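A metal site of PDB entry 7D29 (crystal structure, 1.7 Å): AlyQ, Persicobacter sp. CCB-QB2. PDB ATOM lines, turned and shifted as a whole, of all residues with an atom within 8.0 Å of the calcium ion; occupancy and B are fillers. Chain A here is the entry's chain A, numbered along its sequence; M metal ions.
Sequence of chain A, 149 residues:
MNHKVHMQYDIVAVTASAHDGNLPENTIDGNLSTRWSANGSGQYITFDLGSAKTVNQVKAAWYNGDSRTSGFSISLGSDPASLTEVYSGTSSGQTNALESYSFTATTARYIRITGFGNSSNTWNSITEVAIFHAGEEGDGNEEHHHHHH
ND2 of Asn 26 lies within hydrogen-bond range of O of Arg 35 (2.9 Å). The backbone NH (N) of Leu 23 lies close to the side-chain amide nitrogen (ND2) of Asn 26. N of Thr 127 is in hydrogen-bond range of O of Ala 61, at 2.8 Å. OD1 of Asn 31 is in hydrogen-bond range of N of Ser 33 (2.9 Å).
The calcium ion is bound by the backbone carbonyl oxygen (O) of Asn 26 (2.2 Å). The backbone carbonyl oxygen (O) of Thr 127 binds the calcium ion (2.3 Å). O of Asn 31 binds the calcium ion, at 2.3 Å. The calcium ion is bound by OG1 of Thr 34 (2.4 Å). The calcium ion is bound by OD1 of Asp 29 (2.6 Å). The backbone carbonyl oxygen (O) of Thr 34 is bound to the calcium ion (2.6 Å).
Of the 19 residues printed, 5 come within 4 Å of the calcium ion.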
ATOM      1  N   LEU A  23     -28.099 -14.825 -13.810  1.00  0.00           N
ATOM      2  CA  LEU A  23     -27.220 -14.658 -14.995  1.00  0.00           C
ATOM      3  C   LEU A  23     -25.783 -15.071 -14.672  1.00  0.00           C
ATOM      4  O   LEU A  23     -25.296 -14.850 -13.572  1.00  0.00           O
ATOM      5  CB  LEU A  23     -27.240 -13.218 -15.467  1.00  0.00           C
ATOM      6  CG  LEU A  23     -28.550 -12.719 -16.053  1.00  0.00           C
ATOM      7  CD1 LEU A  23     -28.370 -11.278 -16.461  1.00  0.00           C
ATOM      8  CD2 LEU A  23     -28.948 -13.598 -17.204  1.00  0.00           C
ATOM      9  N   PRO A  24     -25.068 -15.570 -15.701  1.00  0.00           N
ATOM     10  CA  PRO A  24     -23.648 -15.863 -15.567  1.00  0.00           C
ATOM     11  C   PRO A  24     -22.822 -14.699 -15.017  1.00  0.00           C
ATOM     12  O   PRO A  24     -21.959 -14.933 -14.148  1.00  0.00           O
ATOM     13  CB  PRO A  24     -23.258 -16.198 -17.010  1.00  0.00           C
ATOM     14  CG  PRO A  24     -24.496 -16.810 -17.592  1.00  0.00           C
ATOM     15  CD  PRO A  24     -25.578 -15.898 -17.050  1.00  0.00           C
ATOM     16  N   GLU A  25     -23.145 -13.451 -15.413  1.00  0.00           N
ATOM     17  CA  GLU A  25     -22.410 -12.247 -14.933  1.00  0.00           C
ATOM     18  C   GLU A  25     -22.530 -12.081 -13.414  1.00  0.00           C
ATOM     19  O   GLU A  25     -21.692 -11.345 -12.820  1.00  0.00           O
ATOM     20  CB  GLU A  25     -22.946 -10.956 -15.585  1.00  0.00           C
ATOM     21  CG  GLU A  25     -24.338 -10.584 -15.061  1.00  0.00           C
ATOM     22  CD  GLU A  25     -25.056  -9.339 -15.552  1.00  0.00           C
ATOM     23  OE1 GLU A  25     -25.394  -9.263 -16.705  1.00  0.00           O
ATOM     24  OE2 GLU A  25     -25.325  -8.465 -14.715  1.00  0.00           O
ATOM     25  N   ASN A  26     -23.500 -12.701 -12.758  1.00  0.00           N
ATOM     26  CA  ASN A  26     -23.646 -12.596 -11.282  1.00  0.00           C
ATOM     27  C   ASN A  26     -22.429 -13.215 -10.585  1.00  0.00           C
ATOM     28  O   ASN A  26     -22.280 -12.973  -9.375  1.00  0.00           O
ATOM     29  CB  ASN A  26     -24.937 -13.203 -10.781  1.00  0.00           C
ATOM     30  CG  ASN A  26     -26.160 -12.437 -11.217  1.00  0.00           C
ATOM     31  OD1 ASN A  26     -26.064 -11.324 -11.729  1.00  0.00           O
ATOM     32  ND2 ASN A  26     -27.312 -13.040 -10.988  1.00  0.00           N
ATOM     33  N   THR A  27     -21.637 -14.057 -11.254  1.00  0.00           N
ATOM     34  CA  THR A  27     -20.431 -14.660 -10.641  1.00  0.00           C
ATOM     35  C   THR A  27     -19.300 -13.651 -10.531  1.00  0.00           C
ATOM     36  O   THR A  27     -18.283 -13.981  -9.834  1.00  0.00           O
ATOM     37  CB  THR A  27     -19.967 -15.925 -11.390  1.00  0.00           C
ATOM     38  OG1 THR A  27     -19.655 -15.598 -12.754  1.00  0.00           O
ATOM     39  CG2 THR A  27     -20.997 -17.027 -11.307  1.00  0.00           C
ATOM     40  N   ILE A  28     -19.358 -12.515 -11.221  1.00  0.00           N
ATOM     41  CA  ILE A  28     -18.201 -11.557 -11.191  1.00  0.00           C
ATOM     42  C   ILE A  28     -18.651 -10.170 -10.695  1.00  0.00           C
ATOM     43  O   ILE A  28     -18.019  -9.183 -11.087  1.00  0.00           O
ATOM     44  CB  ILE A  28     -17.534 -11.543 -12.587  1.00  0.00           C
ATOM     45  CG1 ILE A  28     -18.480 -11.034 -13.696  1.00  0.00           C
ATOM     46  CG2 ILE A  28     -16.959 -12.935 -12.923  1.00  0.00           C
ATOM     47  CD1 ILE A  28     -17.797 -10.720 -15.036  1.00  0.00           C
ATOM     48  N   ASP A  29     -19.692 -10.104  -9.864  1.00  0.00           N
ATOM     49  CA  ASP A  29     -20.250  -8.813  -9.394  1.00  0.00           C
ATOM     50  C   ASP A  29     -19.751  -8.547  -7.980  1.00  0.00           C
ATOM     51  O   ASP A  29     -20.068  -7.473  -7.393  1.00  0.00           O
ATOM     52  CB  ASP A  29     -21.768  -8.755  -9.504  1.00  0.00           C
ATOM     53  CG  ASP A  29     -22.539  -9.687  -8.609  1.00  0.00           C
ATOM     54  OD1 ASP A  29     -21.889 -10.520  -7.903  1.00  0.00           O
ATOM     55  OD2 ASP A  29     -23.781  -9.644  -8.690  1.00  0.00           O
ATOM     56  N   GLY A  30     -18.980  -9.455  -7.412  1.00  0.00           N
ATOM     57  CA  GLY A  30     -18.458  -9.207  -6.049  1.00  0.00           C
ATOM     58  C   GLY A  30     -19.467  -9.457  -4.946  1.00  0.00           C
ATOM     59  O   GLY A  30     -19.150  -9.153  -3.806  1.00  0.00           O
ATOM     60  N   ASN A  31     -20.624 -10.030  -5.253  1.00  0.00           N
ATOM     61  CA  ASN A  31     -21.751 -10.133  -4.324  1.00  0.00           C
ATOM     62  C   ASN A  31     -22.062 -11.588  -4.031  1.00  0.00           C
ATOM     63  O   ASN A  31     -22.504 -12.283  -4.964  1.00  0.00           O
ATOM     64  CB  ASN A  31     -22.974  -9.440  -4.924  1.00  0.00           C
ATOM     65  CG  ASN A  31     -24.055  -9.202  -3.902  1.00  0.00           C
ATOM     66  OD1 ASN A  31     -24.089  -9.835  -2.840  1.00  0.00           O
ATOM     67  ND2 ASN A  31     -24.926  -8.264  -4.224  1.00  0.00           N
ATOM     68  N   LEU A  32     -21.920 -12.025  -2.788  1.00  0.00           N
ATOM     69  CA  LEU A  32     -22.222 -13.437  -2.481  1.00  0.00           C
ATOM     70  C   LEU A  32     -23.729 -13.706  -2.459  1.00  0.00           C
ATOM     71  O   LEU A  32     -24.097 -14.887  -2.352  1.00  0.00           O
ATOM     72  CB  LEU A  32     -21.581 -13.844  -1.150  1.00  0.00           C
ATOM     73  CG  LEU A  32     -20.053 -13.865  -1.189  1.00  0.00           C
ATOM     74  CD1 LEU A  32     -19.508 -13.936   0.208  1.00  0.00           C
ATOM     75  CD2 LEU A  32     -19.515 -15.040  -2.021  1.00  0.00           C
ATOM     76  N   SER A  33     -24.543 -12.676  -2.554  1.00  0.00           N
ATOM     77  CA  SER A  33     -26.021 -12.779  -2.495  1.00  0.00           C
ATOM     78  C   SER A  33     -26.617 -12.938  -3.894  1.00  0.00           C
ATOM     79  O   SER A  33     -27.838 -13.116  -3.968  1.00  0.00           O
ATOM     80  CB  SER A  33     -26.634 -11.572  -1.790  1.00  0.00           C
ATOM     81  OG  SER A  33     -26.396 -11.670  -0.401  1.00  0.00           O
ATOM     82  N   THR A  34     -25.807 -12.869  -4.943  1.00  0.00           N
ATOM     83  CA  THR A  34     -26.276 -13.099  -6.332  1.00  0.00           C
ATOM     84  C   THR A  34     -25.550 -14.308  -6.927  1.00  0.00           C
ATOM     85  O   THR A  34     -24.364 -14.540  -6.572  1.00  0.00           O
ATOM     86  CB  THR A  34     -26.039 -11.894  -7.230  1.00  0.00           C
ATOM     87  OG1 THR A  34     -24.626 -11.737  -7.371  1.00  0.00           O
ATOM     88  CG2 THR A  34     -26.660 -10.628  -6.661  1.00  0.00           C
ATOM     89  N   ARG A  35     -26.191 -14.994  -7.829  1.00  0.00           N
ATOM     90  CA  ARG A  35     -25.640 -16.255  -8.359  1.00  0.00           C
ATOM     91  C   ARG A  35     -25.936 -16.426  -9.834  1.00  0.00           C
ATOM     92  O   ARG A  35     -26.886 -15.798 -10.364  1.00  0.00           O
ATOM     93  CB  ARG A  35     -26.211 -17.465  -7.612  1.00  0.00           C
ATOM     94  CG  ARG A  35     -27.709 -17.687  -7.888  1.00  0.00           C
ATOM     95  CD  ARG A  35     -28.284 -18.754  -6.986  1.00  0.00           C
ATOM     96  NE  ARG A  35     -29.678 -19.062  -7.323  1.00  0.00           N
ATOM     97  CZ  ARG A  35     -30.747 -18.569  -6.702  1.00  0.00           C
ATOM     98  NH1 ARG A  35     -30.628 -17.725  -5.691  1.00  0.00           N
ATOM     99  NH2 ARG A  35     -31.957 -18.937  -7.128  1.00  0.00           N
ATOM    100  N   TRP A  36     -25.141 -17.283 -10.461  1.00  0.00           N
ATOM    101  CA  TRP A  36     -25.522 -18.019 -11.678  1.00  0.00           C
ATOM    102  C   TRP A  36     -26.170 -19.341 -11.279  1.00  0.00           C
ATOM    103  O   TRP A  36     -25.647 -20.005 -10.392  1.00  0.00           O
ATOM    104  CB  TRP A  36     -24.280 -18.269 -12.548  1.00  0.00           C
ATOM    105  CG  TRP A  36     -24.497 -19.276 -13.638  1.00  0.00           C
ATOM    106  CD1 TRP A  36     -25.283 -19.109 -14.735  1.00  0.00           C
ATOM    107  CD2 TRP A  36     -23.928 -20.590 -13.737  1.00  0.00           C
ATOM    108  NE1 TRP A  36     -25.289 -20.239 -15.477  1.00  0.00           N
ATOM    109  CE2 TRP A  36     -24.434 -21.163 -14.936  1.00  0.00           C
ATOM    110  CE3 TRP A  36     -23.093 -21.384 -12.929  1.00  0.00           C
ATOM    111  CZ2 TRP A  36     -24.050 -22.433 -15.387  1.00  0.00           C
ATOM    112  CZ3 TRP A  36     -22.690 -22.609 -13.394  1.00  0.00           C
ATOM    113  CH2 TRP A  36     -23.221 -23.156 -14.564  1.00  0.00           C
ATOM    114  N   ALA A  61     -17.175 -19.577  -5.121  1.00  0.00           N
ATOM    115  CA  ALA A  61     -18.077 -19.532  -3.956  1.00  0.00           C
ATOM    116  C   ALA A  61     -19.378 -20.161  -4.401  1.00  0.00           C
ATOM    117  O   ALA A  61     -19.916 -19.760  -5.408  1.00  0.00           O
ATOM    118  CB  ALA A  61     -18.344 -18.124  -3.463  1.00  0.00           C
ATOM    119  N   ILE A 126     -23.555 -20.926  -8.451  1.00  0.00           N
ATOM    120  CA  ILE A 126     -22.239 -20.329  -8.089  1.00  0.00           C
ATOM    121  C   ILE A 126     -22.488 -18.852  -7.825  1.00  0.00           C
ATOM    122  O   ILE A 126     -23.042 -18.139  -8.722  1.00  0.00           O
ATOM    123  CB  ILE A 126     -21.199 -20.555  -9.213  1.00  0.00           C
ATOM    124  CG1 ILE A 126     -20.944 -22.062  -9.393  1.00  0.00           C
ATOM    125  CG2 ILE A 126     -19.875 -19.878  -8.876  1.00  0.00           C
ATOM    126  CD1 ILE A 126     -20.001 -22.394 -10.505  1.00  0.00           C
ATOM    127  N   THR A 127     -22.000 -18.342  -6.685  1.00  0.00           N
ATOM    128  CA  THR A 127     -22.193 -16.930  -6.372  1.00  0.00           C
ATOM    129  C   THR A 127     -21.027 -16.029  -6.786  1.00  0.00           C
ATOM    130  O   THR A 127     -21.269 -14.830  -7.062  1.00  0.00           O
ATOM    131  CB  THR A 127     -22.439 -16.770  -4.866  1.00  0.00           C
ATOM    132  OG1 THR A 127     -21.277 -17.208  -4.164  1.00  0.00           O
ATOM    133  CG2 THR A 127     -23.664 -17.512  -4.426  1.00  0.00           C
ATOM    134  N   GLU A 128     -19.816 -16.550  -6.867  1.00  0.00           N
ATOM    135  CA  GLU A 128     -18.620 -15.749  -7.223  1.00  0.00           C
ATOM    136  C   GLU A 128     -17.544 -16.675  -7.764  1.00  0.00           C
ATOM    137  O   GLU A 128     -17.423 -17.781  -7.276  1.00  0.00           O
ATOM    138  CB  GLU A 128     -18.030 -14.989  -6.025  1.00  0.00           C
ATOM    139  CG  GLU A 128     -17.043 -13.848  -6.343  1.00  0.00           C
ATOM    140  CD  GLU A 128     -16.633 -13.031  -5.105  1.00  0.00           C
ATOM    141  OE1 GLU A 128     -16.923 -13.503  -3.965  1.00  0.00           O
ATOM    142  OE2 GLU A 128     -16.047 -11.935  -5.233  1.00  0.00           O
ATOM    143  N   VAL A 129     -16.800 -16.175  -8.733  1.00  0.00           N
ATOM    144  CA  VAL A 129     -15.597 -16.875  -9.246  1.00  0.00           C
ATOM    145  C   VAL A 129     -14.483 -15.836  -9.352  1.00  0.00           C
ATOM    146  O   VAL A 129     -14.712 -14.671  -9.769  1.00  0.00           O
ATOM    147  CB  VAL A 129     -15.862 -17.539 -10.606  1.00  0.00           C
ATOM    148  CG1 VAL A 129     -14.592 -18.071 -11.207  1.00  0.00           C
ATOM    149  CG2 VAL A 129     -16.898 -18.645 -10.486  1.00  0.00           C
HETATM  150 CA    CA M   1     -22.486 -12.896  -7.188  1.00  0.00          CA
